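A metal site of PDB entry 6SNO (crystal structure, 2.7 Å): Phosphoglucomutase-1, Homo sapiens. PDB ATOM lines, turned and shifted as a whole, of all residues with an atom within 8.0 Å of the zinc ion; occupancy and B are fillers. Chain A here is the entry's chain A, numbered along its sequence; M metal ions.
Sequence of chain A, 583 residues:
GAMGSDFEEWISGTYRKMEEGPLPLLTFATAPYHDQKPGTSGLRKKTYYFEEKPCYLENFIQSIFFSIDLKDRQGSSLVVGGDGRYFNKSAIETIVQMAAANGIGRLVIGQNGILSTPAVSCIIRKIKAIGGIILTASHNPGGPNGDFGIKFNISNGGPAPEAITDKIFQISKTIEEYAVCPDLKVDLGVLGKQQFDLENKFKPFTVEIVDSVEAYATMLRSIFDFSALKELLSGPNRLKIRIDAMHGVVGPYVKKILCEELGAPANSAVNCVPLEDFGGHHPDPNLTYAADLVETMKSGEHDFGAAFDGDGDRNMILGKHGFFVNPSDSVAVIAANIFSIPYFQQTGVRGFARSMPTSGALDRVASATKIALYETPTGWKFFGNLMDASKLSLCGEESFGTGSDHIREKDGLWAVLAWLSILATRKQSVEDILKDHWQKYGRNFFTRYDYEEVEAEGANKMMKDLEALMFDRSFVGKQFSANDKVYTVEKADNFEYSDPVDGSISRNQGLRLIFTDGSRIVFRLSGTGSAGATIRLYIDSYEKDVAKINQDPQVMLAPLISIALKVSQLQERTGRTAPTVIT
NE of Arg 314 sits close to O2P of SEP 138, at 2.8 Å. O of SEP 138 is in hydrogen-bond range of the guanidinium group of Arg 85. N of SEP 138 sits at hydrogen-bond distance from the side-chain hydroxyl of Thr 136 (2.7 Å). O1P of SEP 138 lies within salt-bridge range of NH1 of Arg 44 (3.6 Å). O1P of SEP 138 sits at hydrogen-bond distance from ND1 of His 139, at 3.4 Å. The side-chain carboxylate of Asp 311 sits at hydrogen-bond distance from the side-chain hydroxyl of Thr 117 (2.8 Å). NH1 of Arg 314 lies within salt-bridge range of OD1 of Asp 284 (2.9 Å). N of Arg 314 lies within hydrogen-bond range of OD1 of Asp 309 (3.0 Å).
Arg 314 touches the zinc ion. Of the 27 residues printed, 5 come within 4 Å of the zinc ion.
The zinc ion is bound by the side-chain carboxylate (OD2) of Asp 309 (2.0 Å). OD1 of Asp 313 is bound to the zinc ion (2.0 Å). The side-chain carboxylate (OD1) of Asp 311 binds the zinc ion, 2.0 Å away. OG of SEP 138 is bound to the zinc ion (2.4 Å). The zinc ion is bound by O2P of SEP 138, at 2.5 Å.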
ATOM      1  N   SER A  41      22.248   9.223  -1.692  1.00  0.00           N
ATOM      2  CA  SER A  41      22.472   8.298  -0.592  1.00  0.00           C
ATOM      3  C   SER A  41      22.248   6.867  -1.054  1.00  0.00           C
ATOM      4  O   SER A  41      21.615   6.055  -0.374  1.00  0.00           O
ATOM      5  CB  SER A  41      21.551   8.627   0.581  1.00  0.00           C
ATOM      6  OG  SER A  41      21.527  10.016   0.838  1.00  0.00           O
ATOM      7  N   ARG A  44      17.452   3.795  -2.930  1.00  0.00           N
ATOM      8  CA  ARG A  44      16.477   3.579  -1.884  1.00  0.00           C
ATOM      9  C   ARG A  44      15.097   3.400  -2.487  1.00  0.00           C
ATOM     10  O   ARG A  44      14.650   4.233  -3.293  1.00  0.00           O
ATOM     11  CB  ARG A  44      16.481   4.736  -0.884  1.00  0.00           C
ATOM     12  CG  ARG A  44      17.868   5.175  -0.459  1.00  0.00           C
ATOM     13  CD  ARG A  44      17.965   5.294   1.040  1.00  0.00           C
ATOM     14  NE  ARG A  44      17.251   6.476   1.535  1.00  0.00           N
ATOM     15  CZ  ARG A  44      17.835   7.487   2.157  1.00  0.00           C
ATOM     16  NH1 ARG A  44      19.142   7.466   2.385  1.00  0.00           N
ATOM     17  NH2 ARG A  44      17.114   8.524   2.564  1.00  0.00           N
ATOM     18  N   ASP A  83      22.493  -1.269   8.697  1.00  0.00           N
ATOM     19  CA  ASP A  83      21.910  -0.735   9.922  1.00  0.00           C
ATOM     20  C   ASP A  83      20.979  -1.722  10.608  1.00  0.00           C
ATOM     21  O   ASP A  83      20.201  -1.318  11.486  1.00  0.00           O
ATOM     22  CB  ASP A  83      21.176   0.580   9.625  1.00  0.00           C
ATOM     23  CG  ASP A  83      20.071   0.420   8.593  1.00  0.00           C
ATOM     24  OD1 ASP A  83      19.636  -0.722   8.313  1.00  0.00           O
ATOM     25  OD2 ASP A  83      19.628   1.451   8.056  1.00  0.00           O
ATOM     26  N   ARG A  85      18.283  -3.225   9.600  1.00  0.00           N
ATOM     27  CA  ARG A  85      16.862  -3.126   9.306  1.00  0.00           C
ATOM     28  C   ARG A  85      16.366  -4.397   8.645  1.00  0.00           C
ATOM     29  O   ARG A  85      17.135  -5.296   8.305  1.00  0.00           O
ATOM     30  CB  ARG A  85      16.573  -1.896   8.433  1.00  0.00           C
ATOM     31  CG  ARG A  85      16.814  -2.101   6.955  1.00  0.00           C
ATOM     32  CD  ARG A  85      16.467  -0.847   6.161  1.00  0.00           C
ATOM     33  NE  ARG A  85      17.067   0.355   6.733  1.00  0.00           N
ATOM     34  CZ  ARG A  85      16.393   1.447   7.064  1.00  0.00           C
ATOM     35  NH1 ARG A  85      15.087   1.503   6.867  1.00  0.00           N
ATOM     36  NH2 ARG A  85      17.029   2.489   7.582  1.00  0.00           N
ATOM     37  N   THR A 117      27.377   3.247   9.156  1.00  0.00           N
ATOM     38  CA  THR A 117      27.995   3.888   7.987  1.00  0.00           C
ATOM     39  C   THR A 117      29.383   4.428   8.273  1.00  0.00           C
ATOM     40  O   THR A 117      30.308   4.128   7.485  1.00  0.00           O
ATOM     41  CB  THR A 117      27.060   4.996   7.461  1.00  0.00           C
ATOM     42  OG1 THR A 117      25.848   4.411   6.974  1.00  0.00           O
ATOM     43  CG2 THR A 117      27.723   5.754   6.338  1.00  0.00           C
ATOM     44  N   PRO A 118      29.636   5.183   9.355  1.00  0.00           N
ATOM     45  CA  PRO A 118      31.022   5.551   9.671  1.00  0.00           C
ATOM     46  C   PRO A 118      31.920   4.346   9.924  1.00  0.00           C
ATOM     47  O   PRO A 118      33.110   4.394   9.611  1.00  0.00           O
ATOM     48  CB  PRO A 118      30.882   6.419  10.922  1.00  0.00           C
ATOM     49  CG  PRO A 118      29.485   6.903  10.887  1.00  0.00           C
ATOM     50  CD  PRO A 118      28.706   5.762  10.342  1.00  0.00           C
ATOM     51  N   THR A 136      21.461   0.250   4.117  1.00  0.00           N
ATOM     52  CA  THR A 136      20.782   1.234   4.951  1.00  0.00           C
ATOM     53  C   THR A 136      19.873   2.107   4.098  1.00  0.00           C
ATOM     54  O   THR A 136      20.117   2.315   2.909  1.00  0.00           O
ATOM     55  CB  THR A 136      21.761   2.128   5.712  1.00  0.00           C
ATOM     56  OG1 THR A 136      21.039   3.171   6.373  1.00  0.00           O
ATOM     57  CG2 THR A 136      22.754   2.753   4.747  1.00  0.00           C
ATOM     58  N   ALA A 137      18.817   2.600   4.726  1.00  0.00           N
ATOM     59  CA  ALA A 137      17.957   3.611   4.123  1.00  0.00           C
ATOM     60  C   ALA A 137      18.104   4.906   4.923  1.00  0.00           C
ATOM     61  O   ALA A 137      17.258   5.795   4.851  1.00  0.00           O
ATOM     62  CB  ALA A 137      16.507   3.150   4.073  1.00  0.00           C
ATOM     63  N   SEP A 138      19.193   4.978   5.681  1.00  0.00           N
ATOM     64  CA  SEP A 138      19.491   6.107   6.553  1.00  0.00           C
ATOM     65  CB  SEP A 138      19.741   7.376   5.715  1.00  0.00           C
ATOM     66  OG  SEP A 138      20.236   8.425   6.526  1.00  0.00           O
ATOM     67  C   SEP A 138      18.381   6.356   7.568  1.00  0.00           C
ATOM     68  O   SEP A 138      18.042   5.471   8.360  1.00  0.00           O
ATOM     69  P   SEP A 138      21.058   9.494   5.643  1.00  0.00           P
ATOM     70  O1P SEP A 138      20.070  10.199   4.575  1.00  0.00           O
ATOM     71  O2P SEP A 138      21.671  10.593   6.632  1.00  0.00           O
ATOM     72  O3P SEP A 138      22.258   8.748   4.867  1.00  0.00           O
ATOM     73  N   HIS A 139      17.826   7.556   7.544  1.00  0.00           N
ATOM     74  CA  HIS A 139      16.830   7.962   8.532  1.00  0.00           C
ATOM     75  C   HIS A 139      15.417   7.462   8.199  1.00  0.00           C
ATOM     76  O   HIS A 139      14.488   7.675   8.975  1.00  0.00           O
ATOM     77  CB  HIS A 139      16.809   9.490   8.655  1.00  0.00           C
ATOM     78  CG  HIS A 139      16.379  10.192   7.399  1.00  0.00           C
ATOM     79  ND1 HIS A 139      17.256  10.500   6.381  1.00  0.00           N
ATOM     80  CD2 HIS A 139      15.169  10.649   7.008  1.00  0.00           C
ATOM     81  CE1 HIS A 139      16.593  11.114   5.411  1.00  0.00           C
ATOM     82  NE2 HIS A 139      15.328  11.217   5.767  1.00  0.00           N
ATOM     83  N   ASN A 140      15.281   6.782   7.058  1.00  0.00           N
ATOM     84  CA  ASN A 140      13.976   6.315   6.632  1.00  0.00           C
ATOM     85  C   ASN A 140      13.558   5.075   7.415  1.00  0.00           C
ATOM     86  O   ASN A 140      14.400   4.237   7.767  1.00  0.00           O
ATOM     87  CB  ASN A 140      13.983   6.018   5.138  1.00  0.00           C
ATOM     88  CG  ASN A 140      14.045   7.270   4.286  1.00  0.00           C
ATOM     89  OD1 ASN A 140      14.664   7.286   3.212  1.00  0.00           O
ATOM     90  ND2 ASN A 140      13.420   8.339   4.764  1.00  0.00           N
ATOM     91  N   LYS A 151      23.902   1.313  -0.550  1.00  0.00           N
ATOM     92  CA  LYS A 151      24.839   2.407  -0.754  1.00  0.00           C
ATOM     93  C   LYS A 151      26.208   1.818  -1.070  1.00  0.00           C
ATOM     94  O   LYS A 151      26.716   0.988  -0.309  1.00  0.00           O
ATOM     95  CB  LYS A 151      24.904   3.302   0.494  1.00  0.00           C
ATOM     96  CG  LYS A 151      25.671   4.595   0.309  1.00  0.00           C
ATOM     97  CD  LYS A 151      25.574   5.463   1.552  1.00  0.00           C
ATOM     98  CE  LYS A 151      26.186   6.841   1.322  1.00  0.00           C
ATOM     99  NZ  LYS A 151      25.998   7.750   2.496  1.00  0.00           N
ATOM    100  N   PRO A 283      13.475   6.567  12.619  1.00  0.00           N
ATOM    101  CA  PRO A 283      14.882   6.670  13.022  1.00  0.00           C
ATOM    102  C   PRO A 283      15.545   7.957  12.540  1.00  0.00           C
ATOM    103  O   PRO A 283      16.605   7.905  11.892  1.00  0.00           O
ATOM    104  CB  PRO A 283      15.514   5.432  12.387  1.00  0.00           C
ATOM    105  CG  PRO A 283      14.690   5.191  11.169  1.00  0.00           C
ATOM    106  CD  PRO A 283      13.279   5.583  11.544  1.00  0.00           C
ATOM    107  N   ASP A 284      14.947   9.091  12.853  1.00  0.00           N
ATOM    108  CA  ASP A 284      15.451  10.407  12.465  1.00  0.00           C
ATOM    109  C   ASP A 284      15.580  11.258  13.715  1.00  0.00           C
ATOM    110  O   ASP A 284      14.597  11.407  14.468  1.00  0.00           O
ATOM    111  CB  ASP A 284      14.500  11.075  11.465  1.00  0.00           C
ATOM    112  CG  ASP A 284      15.223  11.914  10.426  1.00  0.00           C
ATOM    113  OD1 ASP A 284      16.435  12.190  10.596  1.00  0.00           O
ATOM    114  OD2 ASP A 284      14.567  12.317   9.441  1.00  0.00           O
ATOM    115  N   PRO A 285      16.747  11.828  14.018  1.00  0.00           N
ATOM    116  CA  PRO A 285      16.878  12.650  15.225  1.00  0.00           C
ATOM    117  C   PRO A 285      16.474  14.090  14.965  1.00  0.00           C
ATOM    118  O   PRO A 285      17.152  14.822  14.221  1.00  0.00           O
ATOM    119  CB  PRO A 285      18.368  12.517  15.571  1.00  0.00           C
ATOM    120  CG  PRO A 285      19.032  12.258  14.274  1.00  0.00           C
ATOM    121  CD  PRO A 285      18.046  11.566  13.374  1.00  0.00           C
ATOM    122  N   PHE A 308      20.652   9.619  17.488  1.00  0.00           N
ATOM    123  CA  PHE A 308      21.248   9.232  16.219  1.00  0.00           C
ATOM    124  C   PHE A 308      20.169   8.769  15.262  1.00  0.00           C
ATOM    125  O   PHE A 308      19.021   8.517  15.653  1.00  0.00           O
ATOM    126  CB  PHE A 308      22.296   8.128  16.418  1.00  0.00           C
ATOM    127  CG  PHE A 308      23.327   8.447  17.455  1.00  0.00           C
ATOM    128  CD1 PHE A 308      24.253   9.455  17.248  1.00  0.00           C
ATOM    129  CD2 PHE A 308      23.383   7.726  18.637  1.00  0.00           C
ATOM    130  CE1 PHE A 308      25.210   9.758  18.203  1.00  0.00           C
ATOM    131  CE2 PHE A 308      24.338   8.022  19.604  1.00  0.00           C
ATOM    132  CZ  PHE A 308      25.245   9.029  19.384  1.00  0.00           C
ATOM    133  N   ASP A 309      20.527   8.650  13.991  1.00  0.00           N
ATOM    134  CA  ASP A 309      19.611   8.148  12.991  1.00  0.00           C
ATOM    135  C   ASP A 309      19.916   6.671  12.719  1.00  0.00           C
ATOM    136  O   ASP A 309      20.683   6.031  13.434  1.00  0.00           O
ATOM    137  CB  ASP A 309      19.657   8.995  11.720  1.00  0.00           C
ATOM    138  CG  ASP A 309      20.925   8.809  10.933  1.00  0.00           C
ATOM    139  OD1 ASP A 309      22.015   8.691  11.545  1.00  0.00           O
ATOM    140  OD2 ASP A 309      20.838   8.781   9.690  1.00  0.00           O
ATOM    141  N   GLY A 310      19.297   6.129  11.669  1.00  0.00           N
ATOM    142  CA  GLY A 310      19.343   4.694  11.447  1.00  0.00           C
ATOM    143  C   GLY A 310      20.749   4.156  11.243  1.00  0.00           C
ATOM    144  O   GLY A 310      21.146   3.167  11.863  1.00  0.00           O
ATOM    145  N   ASP A 311      21.516   4.794  10.368  1.00  0.00           N
ATOM    146  CA  ASP A 311      22.829   4.294   9.985  1.00  0.00           C
ATOM    147  C   ASP A 311      23.972   4.991  10.710  1.00  0.00           C
ATOM    148  O   ASP A 311      25.130   4.603  10.532  1.00  0.00           O
ATOM    149  CB  ASP A 311      23.032   4.394   8.473  1.00  0.00           C
ATOM    150  CG  ASP A 311      22.911   5.815   7.955  1.00  0.00           C
ATOM    151  OD1 ASP A 311      22.046   6.570   8.441  1.00  0.00           O
ATOM    152  OD2 ASP A 311      23.697   6.172   7.049  1.00  0.00           O
ATOM    153  N   GLY A 312      23.689   6.030  11.493  1.00  0.00           N
ATOM    154  CA  GLY A 312      24.664   6.567  12.416  1.00  0.00           C
ATOM    155  C   GLY A 312      25.526   7.720  11.932  1.00  0.00           C
ATOM    156  O   GLY A 312      26.520   8.036  12.593  1.00  0.00           O
ATOM    157  N   ASP A 313      25.177   8.351  10.816  1.00  0.00           N
ATOM    158  CA  ASP A 313      25.941   9.520  10.374  1.00  0.00           C
ATOM    159  C   ASP A 313      25.321  10.837  10.808  1.00  0.00           C
ATOM    160  O   ASP A 313      25.937  11.883  10.606  1.00  0.00           O
ATOM    161  CB  ASP A 313      26.122   9.502   8.845  1.00  0.00           C
ATOM    162  CG  ASP A 313      24.816   9.332   8.096  1.00  0.00           C
ATOM    163  OD1 ASP A 313      23.742   9.285   8.740  1.00  0.00           O
ATOM    164  OD2 ASP A 313      24.869   9.249   6.846  1.00  0.00           O
ATOM    165  N   ARG A 314      24.132  10.815  11.420  1.00  0.00           N
ATOM    166  CA  ARG A 314      23.489  12.024  11.920  1.00  0.00           C
ATOM    167  C   ARG A 314      23.358  11.975  13.433  1.00  0.00           C
ATOM    168  O   ARG A 314      23.388  10.909  14.055  1.00  0.00           O
ATOM    169  CB  ARG A 314      22.110  12.226  11.294  1.00  0.00           C
ATOM    170  CG  ARG A 314      22.089  12.096   9.786  1.00  0.00           C
ATOM    171  CD  ARG A 314      20.668  11.918   9.302  1.00  0.00           C
ATOM    172  NE  ARG A 314      20.423  12.609   8.049  1.00  0.00           N
ATOM    173  CZ  ARG A 314      19.306  13.262   7.768  1.00  0.00           C
ATOM    174  NH1 ARG A 314      18.335  13.313   8.656  1.00  0.00           N
ATOM    175  NH2 ARG A 314      19.170  13.876   6.590  1.00  0.00           N
ATOM    176  N   ASN A 315      23.195  13.159  14.026  1.00  0.00           N
ATOM    177  CA  ASN A 315      23.147  13.285  15.477  1.00  0.00           C
ATOM    178  C   ASN A 315      22.381  14.548  15.860  1.00  0.00           C
ATOM    179  O   ASN A 315      22.398  15.541  15.137  1.00  0.00           O
ATOM    180  CB  ASN A 315      24.555  13.329  16.062  1.00  0.00           C
ATOM    181  CG  ASN A 315      25.222  14.670  15.888  1.00  0.00           C
ATOM    182  OD1 ASN A 315      25.213  15.506  16.794  1.00  0.00           O
ATOM    183  ND2 ASN A 315      25.789  14.896  14.703  1.00  0.00           N
ATOM    184  N   SER A 399      20.974  19.240   8.222  1.00  0.00           N
ATOM    185  CA  SER A 399      20.195  18.019   8.396  1.00  0.00           C
ATOM    186  C   SER A 399      20.806  17.120   9.469  1.00  0.00           C
ATOM    187  O   SER A 399      20.926  15.905   9.268  1.00  0.00           O
ATOM    188  CB  SER A 399      20.087  17.268   7.069  1.00  0.00           C
ATOM    189  OG  SER A 399      21.364  17.102   6.478  1.00  0.00           O
ATOM    190  N   PHE A 400      21.194  17.715  10.599  1.00  0.00           N
ATOM    191  CA  PHE A 400      21.791  16.991  11.715  1.00  0.00           C
ATOM    192  C   PHE A 400      23.042  16.237  11.278  1.00  0.00           C
ATOM    193  O   PHE A 400      23.290  15.106  11.693  1.00  0.00           O
ATOM    194  CB  PHE A 400      20.778  16.048  12.362  1.00  0.00           C
ATOM    195  CG  PHE A 400      19.657  16.778  13.060  1.00  0.00           C
ATOM    196  CD1 PHE A 400      18.582  17.268  12.339  1.00  0.00           C
ATOM    197  CD2 PHE A 400      19.691  16.969  14.432  1.00  0.00           C
ATOM    198  CE1 PHE A 400      17.556  17.938  12.978  1.00  0.00           C
ATOM    199  CE2 PHE A 400      18.664  17.638  15.070  1.00  0.00           C
ATOM    200  CZ  PHE A 400      17.595  18.127  14.341  1.00  0.00           C
ATOM    201  N   GLU A 409      32.652   9.799   5.591  1.00  0.00           N
ATOM    202  CA  GLU A 409      31.228   9.908   5.853  1.00  0.00           C
ATOM    203  C   GLU A 409      31.048  10.744   7.118  1.00  0.00           C
ATOM    204  O   GLU A 409      31.970  10.878   7.924  1.00  0.00           O
ATOM    205  CB  GLU A 409      30.552   8.540   6.026  1.00  0.00           C
ATOM    206  CG  GLU A 409      30.523   7.662   4.787  1.00  0.00           C
ATOM    207  CD  GLU A 409      29.221   7.791   4.008  1.00  0.00           C
ATOM    208  OE1 GLU A 409      28.335   8.539   4.470  1.00  0.00           O
ATOM    209  OE2 GLU A 409      29.096   7.141   2.954  1.00  0.00           O
ATOM    210  N   LYS A 410      29.857  11.308   7.279  1.00  0.00           N
ATOM    211  CA  LYS A 410      29.567  12.003   8.522  1.00  0.00           C
ATOM    212  C   LYS A 410      29.382  10.984   9.648  1.00  0.00           C
ATOM    213  O   LYS A 410      29.137   9.791   9.407  1.00  0.00           O
ATOM    214  CB  LYS A 410      28.339  12.898   8.364  1.00  0.00           C
ATOM    215  CG  LYS A 410      28.513  13.956   7.285  1.00  0.00           C
ATOM    216  CD  LYS A 410      27.715  15.218   7.586  1.00  0.00           C
ATOM    217  CE  LYS A 410      27.960  16.303   6.536  1.00  0.00           C
ATOM    218  NZ  LYS A 410      29.401  16.704   6.457  1.00  0.00           N
HETATM  219 ZN    ZN M   1      21.995   8.551   8.095  1.00  0.00          ZN
